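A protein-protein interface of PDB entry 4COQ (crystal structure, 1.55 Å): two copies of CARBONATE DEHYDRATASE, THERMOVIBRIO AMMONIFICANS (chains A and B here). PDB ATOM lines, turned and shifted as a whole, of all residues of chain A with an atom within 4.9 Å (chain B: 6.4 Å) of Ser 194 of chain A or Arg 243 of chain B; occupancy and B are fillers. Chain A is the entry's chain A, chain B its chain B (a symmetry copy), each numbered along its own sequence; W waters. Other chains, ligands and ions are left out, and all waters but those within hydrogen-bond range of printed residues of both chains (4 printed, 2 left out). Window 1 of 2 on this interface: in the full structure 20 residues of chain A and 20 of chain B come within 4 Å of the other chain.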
ATOM      1  N   ASN A  52      27.110  -9.408 -13.307  1.00  0.00           N
ATOM      2  CA  ASN A  52      26.434  -9.725 -12.038  1.00  0.00           C
ATOM      3  C   ASN A  52      26.762 -11.169 -11.652  1.00  0.00           C
ATOM      4  O   ASN A  52      25.873 -11.990 -11.421  1.00  0.00           O
ATOM      5  CB  ASN A  52      24.915  -9.502 -12.176  1.00  0.00           C
ATOM      6  CG  ASN A  52      24.563  -8.025 -12.411  1.00  0.00           C
ATOM      7  OD1 ASN A  52      24.334  -7.285 -11.460  1.00  0.00           O
ATOM      8  ND2 ASN A  52      24.527  -7.594 -13.658  1.00  0.00           N
ATOM      9  N   ARG A 192      22.345 -10.559   1.381  1.00  0.00           N
ATOM     10  CA  ARG A 192      21.673 -10.887   0.102  1.00  0.00           C
ATOM     11  C   ARG A 192      22.209 -10.051  -1.061  1.00  0.00           C
ATOM     12  O   ARG A 192      22.473  -8.864  -0.913  1.00  0.00           O
ATOM     13  CB  ARG A 192      20.149 -10.691   0.214  1.00  0.00           C
ATOM     14  CG  ARG A 192      19.467 -11.016  -1.114  1.00  0.00           C
ATOM     15  CD  ARG A 192      17.950 -10.973  -1.046  1.00  0.00           C
ATOM     16  NE  ARG A 192      17.396 -11.090  -2.403  1.00  0.00           N
ATOM     17  CZ  ARG A 192      16.096 -11.269  -2.664  1.00  0.00           C
ATOM     18  NH1 ARG A 192      15.227 -11.336  -1.665  1.00  0.00           N
ATOM     19  NH2 ARG A 192      15.667 -11.327  -3.925  1.00  0.00           N
ATOM     20  N   TYR A 193      22.389 -10.700  -2.227  1.00  0.00           N
ATOM     21  CA  TYR A 193      22.719  -9.984  -3.447  1.00  0.00           C
ATOM     22  C   TYR A 193      22.264 -10.831  -4.607  1.00  0.00           C
ATOM     23  O   TYR A 193      21.889 -11.987  -4.413  1.00  0.00           O
ATOM     24  CB  TYR A 193      24.228  -9.687  -3.570  1.00  0.00           C
ATOM     25  CG  TYR A 193      25.099 -10.869  -3.920  1.00  0.00           C
ATOM     26  CD1 TYR A 193      25.480 -11.806  -2.945  1.00  0.00           C
ATOM     27  CD2 TYR A 193      25.552 -11.040  -5.226  1.00  0.00           C
ATOM     28  CE1 TYR A 193      26.303 -12.898  -3.269  1.00  0.00           C
ATOM     29  CE2 TYR A 193      26.365 -12.112  -5.559  1.00  0.00           C
ATOM     30  CZ  TYR A 193      26.707 -13.042  -4.590  1.00  0.00           C
ATOM     31  OH  TYR A 193      27.482 -14.117  -4.940  1.00  0.00           O
ATOM     32  N   SER A 194      22.198 -10.203  -5.766  1.00  0.00           N
ATOM     33  CA  SER A 194      21.794 -10.834  -7.040  1.00  0.00           C
ATOM     34  C   SER A 194      23.038 -11.244  -7.798  1.00  0.00           C
ATOM     35  O   SER A 194      23.896 -10.395  -8.051  1.00  0.00           O
ATOM     36  CB  SER A 194      21.025  -9.794  -7.890  1.00  0.00           C
ATOM     37  OG  SER A 194      20.905 -10.163  -9.274  1.00  0.00           O
ATOM     38  N   GLY A 195      23.115 -12.503  -8.216  1.00  0.00           N
ATOM     39  CA  GLY A 195      24.331 -12.947  -8.834  1.00  0.00           C
ATOM     40  C   GLY A 195      24.112 -14.048  -9.846  1.00  0.00           C
ATOM     41  O   GLY A 195      23.178 -13.994 -10.636  1.00  0.00           O
ATOM     42  N   SER A 196      25.006 -15.037  -9.783  1.00  0.00           N
ATOM     43  CA  SER A 196      25.054 -16.049 -10.855  1.00  0.00           C
ATOM     44  C   SER A 196      25.316 -17.422 -10.251  1.00  0.00           C
ATOM     45  O   SER A 196      25.646 -17.549  -9.085  1.00  0.00           O
ATOM     46  CB  SER A 196      26.161 -15.704 -11.862  1.00  0.00           C
ATOM     47  OG  SER A 196      27.453 -16.068 -11.366  1.00  0.00           O
ATOM     48  N   VAL A 206      20.303 -15.240 -10.336  1.00  0.00           N
ATOM     49  CA  VAL A 206      20.317 -16.145  -9.189  1.00  0.00           C
ATOM     50  C   VAL A 206      20.261 -15.301  -7.906  1.00  0.00           C
ATOM     51  O   VAL A 206      21.030 -14.353  -7.752  1.00  0.00           O
ATOM     52  CB  VAL A 206      21.591 -17.032  -9.174  1.00  0.00           C
ATOM     53  CG1 VAL A 206      21.615 -17.909  -7.937  1.00  0.00           C
ATOM     54  CG2 VAL A 206      21.653 -17.920 -10.425  1.00  0.00           C
ATOM     55  N   ARG A 243      26.253  -3.500  -8.251  1.00  0.00           N
ATOM     56  CA  ARG A 243      25.449  -4.107  -7.189  1.00  0.00           C
ATOM     57  C   ARG A 243      25.831  -3.591  -5.803  1.00  0.00           C
ATOM     58  O   ARG A 243      26.980  -3.182  -5.562  1.00  0.00           O
ATOM     59  CB  ARG A 243      25.619  -5.618  -7.190  1.00  0.00           C
ATOM     60  CG  ARG A 243      25.180  -6.256  -8.497  1.00  0.00           C
ATOM     61  CD  ARG A 243      25.528  -7.747  -8.453  1.00  0.00           C
ATOM     62  NE  ARG A 243      26.948  -7.947  -8.719  1.00  0.00           N
ATOM     63  CZ  ARG A 243      27.520  -9.160  -8.746  1.00  0.00           C
ATOM     64  NH1 ARG A 243      26.784 -10.246  -8.504  1.00  0.00           N
ATOM     65  NH2 ARG A 243      28.806  -9.287  -9.002  1.00  0.00           N
ATOM     66  N   LYS B  51      19.660 -10.764 -17.662  1.00  0.00           N
ATOM     67  CA  LYS B  51      18.723 -10.977 -16.554  1.00  0.00           C
ATOM     68  C   LYS B  51      18.767  -9.796 -15.600  1.00  0.00           C
ATOM     69  O   LYS B  51      18.123  -9.823 -14.552  1.00  0.00           O
ATOM     70  CB  LYS B  51      19.052 -12.287 -15.782  1.00  0.00           C
ATOM     71  CG  LYS B  51      19.044 -13.554 -16.653  1.00  0.00           C
ATOM     72  CD  LYS B  51      17.644 -13.778 -17.202  1.00  0.00           C
ATOM     73  CE  LYS B  51      17.565 -14.976 -18.146  1.00  0.00           C
ATOM     74  NZ  LYS B  51      16.223 -15.057 -18.807  1.00  0.00           N
ATOM     75  N   ASN B  52      19.508  -8.759 -15.978  1.00  0.00           N
ATOM     76  CA  ASN B  52      19.569  -7.557 -15.134  1.00  0.00           C
ATOM     77  C   ASN B  52      19.335  -6.327 -16.016  1.00  0.00           C
ATOM     78  O   ASN B  52      20.134  -5.366 -16.008  1.00  0.00           O
ATOM     79  CB  ASN B  52      20.946  -7.502 -14.436  1.00  0.00           C
ATOM     80  CG  ASN B  52      21.091  -8.601 -13.399  1.00  0.00           C
ATOM     81  OD1 ASN B  52      20.576  -8.488 -12.284  1.00  0.00           O
ATOM     82  ND2 ASN B  52      21.771  -9.689 -13.772  1.00  0.00           N
ATOM     83  N   GLN B  53      18.217  -6.357 -16.746  1.00  0.00           N
ATOM     84  CA  GLN B  53      17.905  -5.337 -17.758  1.00  0.00           C
ATOM     85  C   GLN B  53      17.048  -4.221 -17.184  1.00  0.00           C
ATOM     86  O   GLN B  53      16.407  -4.396 -16.171  1.00  0.00           O
ATOM     87  CB  GLN B  53      17.207  -5.962 -18.975  1.00  0.00           C
ATOM     88  CG  GLN B  53      18.135  -6.898 -19.745  1.00  0.00           C
ATOM     89  CD  GLN B  53      19.074  -6.121 -20.650  1.00  0.00           C
ATOM     90  OE1 GLN B  53      18.642  -5.518 -21.622  1.00  0.00           O
ATOM     91  NE2 GLN B  53      20.348  -6.097 -20.307  1.00  0.00           N
ATOM     92  N   SER B  54      17.071  -3.072 -17.862  1.00  0.00           N
ATOM     93  CA  SER B  54      16.302  -1.874 -17.506  1.00  0.00           C
ATOM     94  C   SER B  54      15.501  -1.486 -18.732  1.00  0.00           C
ATOM     95  O   SER B  54      15.887  -1.835 -19.869  1.00  0.00           O
ATOM     96  CB  SER B  54      17.258  -0.727 -17.173  1.00  0.00           C
ATOM     97  OG  SER B  54      17.996  -1.060 -16.001  1.00  0.00           O
ATOM     98  N   PRO B  55      14.386  -0.762 -18.548  1.00  0.00           N
ATOM     99  CA  PRO B  55      13.860  -0.264 -17.276  1.00  0.00           C
ATOM    100  C   PRO B  55      13.036  -1.377 -16.616  1.00  0.00           C
ATOM    101  O   PRO B  55      12.877  -2.450 -17.190  1.00  0.00           O
ATOM    102  CB  PRO B  55      12.941   0.869 -17.734  1.00  0.00           C
ATOM    103  CG  PRO B  55      12.356   0.349 -19.032  1.00  0.00           C
ATOM    104  CD  PRO B  55      13.533  -0.359 -19.681  1.00  0.00           C
ATOM    105  N   ILE B  56      12.546  -1.116 -15.408  1.00  0.00           N
ATOM    106  CA  ILE B  56      11.719  -2.071 -14.672  1.00  0.00           C
ATOM    107  C   ILE B  56      10.469  -1.394 -14.120  1.00  0.00           C
ATOM    108  O   ILE B  56      10.387  -0.169 -14.085  1.00  0.00           O
ATOM    109  CB  ILE B  56      12.518  -2.682 -13.491  1.00  0.00           C
ATOM    110  CG1 ILE B  56      12.985  -1.583 -12.529  1.00  0.00           C
ATOM    111  CG2 ILE B  56      13.696  -3.502 -13.993  1.00  0.00           C
ATOM    112  CD1 ILE B  56      13.494  -2.096 -11.196  1.00  0.00           C
ATOM    113  N   TYR B 193      18.806   0.352  -8.063  1.00  0.00           N
ATOM    114  CA  TYR B 193      18.921  -1.044  -8.459  1.00  0.00           C
ATOM    115  C   TYR B 193      20.038  -1.148  -9.493  1.00  0.00           C
ATOM    116  O   TYR B 193      20.545  -0.132  -9.988  1.00  0.00           O
ATOM    117  CB  TYR B 193      17.591  -1.593  -8.998  1.00  0.00           C
ATOM    118  CG  TYR B 193      17.198  -1.111 -10.377  1.00  0.00           C
ATOM    119  CD1 TYR B 193      16.614   0.143 -10.596  1.00  0.00           C
ATOM    120  CD2 TYR B 193      17.387  -1.960 -11.483  1.00  0.00           C
ATOM    121  CE1 TYR B 193      16.239   0.550 -11.883  1.00  0.00           C
ATOM    122  CE2 TYR B 193      17.022  -1.581 -12.749  1.00  0.00           C
ATOM    123  CZ  TYR B 193      16.458  -0.331 -12.959  1.00  0.00           C
ATOM    124  OH  TYR B 193      16.116   0.048 -14.232  1.00  0.00           O
ATOM    125  N   SER B 194      20.453  -2.390  -9.754  1.00  0.00           N
ATOM    126  CA  SER B 194      21.513  -2.707 -10.712  1.00  0.00           C
ATOM    127  C   SER B 194      20.836  -3.082 -12.029  1.00  0.00           C
ATOM    128  O   SER B 194      20.032  -3.990 -12.033  1.00  0.00           O
ATOM    129  CB  SER B 194      22.324  -3.900 -10.167  1.00  0.00           C
ATOM    130  OG  SER B 194      23.125  -4.493 -11.184  1.00  0.00           O
ATOM    131  N   GLY B 195      21.164  -2.383 -13.113  1.00  0.00           N
ATOM    132  CA  GLY B 195      20.466  -2.659 -14.373  1.00  0.00           C
ATOM    133  C   GLY B 195      21.346  -2.478 -15.587  1.00  0.00           C
ATOM    134  O   GLY B 195      22.523  -2.844 -15.584  1.00  0.00           O
ATOM    135  N   SER B 196      20.768  -1.894 -16.631  1.00  0.00           N
ATOM    136  CA  SER B 196      21.412  -1.842 -17.923  1.00  0.00           C
ATOM    137  C   SER B 196      21.105  -0.510 -18.595  1.00  0.00           C
ATOM    138  O   SER B 196      20.236   0.252 -18.135  1.00  0.00           O
ATOM    139  CB  SER B 196      20.874  -2.975 -18.813  1.00  0.00           C
ATOM    140  OG  SER B 196      19.535  -2.700 -19.302  1.00  0.00           O
ATOM    141  N   GLN B 238      11.312  -4.671 -18.049  1.00  0.00           N
ATOM    142  CA  GLN B 238      11.999  -5.971 -18.056  1.00  0.00           C
ATOM    143  C   GLN B 238      11.847  -6.618 -16.694  1.00  0.00           C
ATOM    144  O   GLN B 238      11.685  -5.903 -15.692  1.00  0.00           O
ATOM    145  CB  GLN B 238      13.487  -5.738 -18.353  1.00  0.00           C
ATOM    146  CG  GLN B 238      13.731  -4.962 -19.636  1.00  0.00           C
ATOM    147  CD  GLN B 238      13.377  -5.768 -20.861  1.00  0.00           C
ATOM    148  OE1 GLN B 238      13.803  -6.919 -20.997  1.00  0.00           O
ATOM    149  NE2 GLN B 238      12.577  -5.178 -21.756  1.00  0.00           N
ATOM    150  N   PRO B 239      11.893  -7.970 -16.628  1.00  0.00           N
ATOM    151  CA  PRO B 239      11.706  -8.729 -15.387  1.00  0.00           C
ATOM    152  C   PRO B 239      12.778  -8.410 -14.369  1.00  0.00           C
ATOM    153  O   PRO B 239      13.940  -8.258 -14.727  1.00  0.00           O
ATOM    154  CB  PRO B 239      11.844 -10.199 -15.828  1.00  0.00           C
ATOM    155  CG  PRO B 239      11.561 -10.195 -17.273  1.00  0.00           C
ATOM    156  CD  PRO B 239      11.957  -8.840 -17.818  1.00  0.00           C
ATOM    157  N   LEU B 240      12.363  -8.243 -13.119  1.00  0.00           N
ATOM    158  CA  LEU B 240      13.284  -7.980 -12.036  1.00  0.00           C
ATOM    159  C   LEU B 240      14.241  -9.162 -11.834  1.00  0.00           C
ATOM    160  O   LEU B 240      15.414  -8.976 -11.490  1.00  0.00           O
ATOM    161  CB  LEU B 240      12.477  -7.695 -10.774  1.00  0.00           C
ATOM    162  CG  LEU B 240      13.157  -7.044  -9.585  1.00  0.00           C
ATOM    163  CD1 LEU B 240      13.760  -5.700  -9.947  1.00  0.00           C
ATOM    164  CD2 LEU B 240      12.117  -6.873  -8.495  1.00  0.00           C
ATOM    165  N   ASN B 241      13.727 -10.380 -12.049  1.00  0.00           N
ATOM    166  CA  ASN B 241      14.507 -11.597 -11.826  1.00  0.00           C
ATOM    167  C   ASN B 241      14.991 -11.698 -10.376  1.00  0.00           C
ATOM    168  O   ASN B 241      14.148 -11.662  -9.478  1.00  0.00           O
ATOM    169  CB  ASN B 241      15.604 -11.760 -12.881  1.00  0.00           C
ATOM    170  CG  ASN B 241      15.017 -11.922 -14.273  1.00  0.00           C
ATOM    171  OD1 ASN B 241      14.063 -12.702 -14.467  1.00  0.00           O
ATOM    172  ND2 ASN B 241      15.542 -11.155 -15.248  1.00  0.00           N
ATOM    173  N   ALA B 242      16.305 -11.810 -10.131  1.00  0.00           N
ATOM    174  CA  ALA B 242      16.821 -11.949  -8.764  1.00  0.00           C
ATOM    175  C   ALA B 242      16.937 -10.666  -7.994  1.00  0.00           C
ATOM    176  O   ALA B 242      17.244 -10.695  -6.795  1.00  0.00           O
ATOM    177  CB  ALA B 242      18.166 -12.653  -8.778  1.00  0.00           C
ATOM    178  N   ARG B 243      16.724  -9.532  -8.664  1.00  0.00           N
ATOM    179  CA  ARG B 243      17.029  -8.247  -8.052  1.00  0.00           C
ATOM    180  C   ARG B 243      16.021  -7.797  -7.026  1.00  0.00           C
ATOM    181  O   ARG B 243      14.811  -8.105  -7.128  1.00  0.00           O
ATOM    182  CB  ARG B 243      17.132  -7.161  -9.134  1.00  0.00           C
ATOM    183  CG  ARG B 243      18.265  -7.429 -10.107  1.00  0.00           C
ATOM    184  CD  ARG B 243      18.264  -6.456 -11.260  1.00  0.00           C
ATOM    185  NE  ARG B 243      17.186  -6.760 -12.226  1.00  0.00           N
ATOM    186  CZ  ARG B 243      16.942  -6.020 -13.303  1.00  0.00           C
ATOM    187  NH1 ARG B 243      17.700  -4.946 -13.538  1.00  0.00           N
ATOM    188  NH2 ARG B 243      15.949  -6.343 -14.136  1.00  0.00           N
ATOM    189  N   LYS B 244      16.528  -7.050  -6.047  1.00  0.00           N
ATOM    190  CA  LYS B 244      15.693  -6.196  -5.220  1.00  0.00           C
ATOM    191  C   LYS B 244      15.966  -4.744  -5.564  1.00  0.00           C
ATOM    192  O   LYS B 244      17.115  -4.369  -5.840  1.00  0.00           O
ATOM    193  CB  LYS B 244      15.948  -6.431  -3.733  1.00  0.00           C
ATOM    194  CG  LYS B 244      15.497  -7.805  -3.248  1.00  0.00           C
ATOM    195  CD  LYS B 244      14.042  -8.151  -3.571  1.00  0.00           C
ATOM    196  CE  LYS B 244      13.131  -7.801  -2.416  1.00  0.00           C
ATOM    197  NZ  LYS B 244      11.727  -8.277  -2.621  1.00  0.00           N
ATOM    198  N   VAL B 245      14.928  -3.922  -5.517  1.00  0.00           N
ATOM    199  CA  VAL B 245      15.098  -2.496  -5.623  1.00  0.00           C
ATOM    200  C   VAL B 245      15.189  -1.995  -4.180  1.00  0.00           C
ATOM    201  O   VAL B 245      14.411  -2.442  -3.346  1.00  0.00           O
ATOM    202  CB  VAL B 245      13.872  -1.851  -6.280  1.00  0.00           C
ATOM    203  CG1 VAL B 245      14.005  -0.343  -6.309  1.00  0.00           C
ATOM    204  CG2 VAL B 245      13.707  -2.395  -7.704  1.00  0.00           C
HETATM  205  O   HOH W   1      23.520  -4.789 -13.943  1.00  0.00           O
HETATM  206  O   HOH W   2      26.398  -5.104 -11.926  1.00  0.00           O
HETATM  207  O   HOH W   3      21.934  -7.428 -10.062  1.00  0.00           O
HETATM  208  O   HOH W   4      21.893 -11.665 -11.512  1.00  0.00           O
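The side-chain amide nitrogen of Asn 52 of chain A lies close to the side-chain amide nitrogen of Asn 52 of chain B, 3.5 Å away.
OD1 of Asn 52 of chain A lies within hydrogen-bond range of OG of Ser 194 of chain B (3.1 Å).
The guanidinium group (NH2) of Arg 192 of chain A lies within hydrogen-bond range of the backbone carbonyl oxygen (O) of Ala 242 of chain B, at 3.3 Å.
OG of Ser 194 of chain A is in hydrogen-bond range of OD1 of Asn 52 of chain B (3.5 Å).
Printed residues of chain B that touch a printed residue of chain A: Asn 52, Ser 194, Ala 242, Arg 243 and Lys 244.
Hydrophobic or aromatic side chains of chain B within 4 Å of the printed part of chain A: Ala 242.
Along chain B the printed residues that touch a printed residue of chain A span positions 52 to 244.
Among the printed residues, 9 pairs touch across the chains.
Asn 52 of chain B touches its own counterpart, Asn 52 of chain A.
Asn 52 of chain A touches Ser 194 of chain B, and with the chains exchanged Ser 194 of chain A touches Asn 52 of chain B.
Ser 194 of chain A touches Arg 243 of chain B, and with the chains exchanged Arg 243 of chain A touches Ser 194 of chain B.
Positions printed for both chains: 52, 193, 194, 195, 196 and 243.
Of the 9 pairs that touch across the chains among the printed residues, 5 have their exchanged pair printed and touching as well.
Printed residues of chain A within 4 Å of Lys 244 of chain B: Arg 192 (3.6 Å).
Printed residues of chain A within 4 Å of Ser 194 of chain B: Asn 52 (3.1 Å) and Arg 243 (3.8 Å).
Gly 195 of chain A touches none of the printed residues of chain B.
Among the printed residues, pairs that only touch across the chains: Val 206 of chain A with Ala 242 of chain B, Arg 192 of chain A with Lys 244 of chain B, Ser 194 of chain A with Ala 242 of chain B, Arg 243 of chain A with Ser 194 of chain B and Ser 194 of chain A with Arg 243 of chain B.
Water W1 lies within hydrogen-bond range of the backbone carbonyl oxygen of Gly 195 of chain B, the side-chain hydroxyl of Ser 194 of chain B and the side-chain amide nitrogen of Asn 52 of chain A.
Water W3 lies within hydrogen-bond range of OD1 of Asn 52 of chain A, OD1 of Asn 52 of chain B, OG of Ser 194 of chain A and OG of Ser 194 of chain B.
Water W4 lies within hydrogen-bond range of O of Gly 195 of chain A, OG of Ser 194 of chain A and ND2 of Asn 52 of chain B.
Water W2 bridges the side-chain amide oxygen (OD1) of Asn 52 of chain A (3.0 Å) and the side-chain hydroxyl (OG) of Ser 194 of chain B (3.4 Å).
The backbone carbonyl oxygen (O) of Ser 194 of chain A sits at hydrogen-bond distance from the guanidinium group (NH1) of Arg 243 of chain A (2.9 Å).
N of Gly 195 of chain A is in hydrogen-bond range of O of Val 206 of chain A, at 2.8 Å.
NH1 of Arg 243 of chain B lies close to O of Asn 52 of chain B (3.5 Å).
The guanidinium group (NH2) of Arg 243 of chain B sits at hydrogen-bond distance from the backbone carbonyl oxygen (O) of Gln 53 of chain B (2.9 Å).
O of Ser 194 of chain B is in hydrogen-bond range of NH1 of Arg 243 of chain B, at 2.9 Å.
The backbone carbonyl oxygen of Leu 240 of chain B is in hydrogen-bond range of the guanidinium group of Arg 243 of chain B (2.9 Å).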
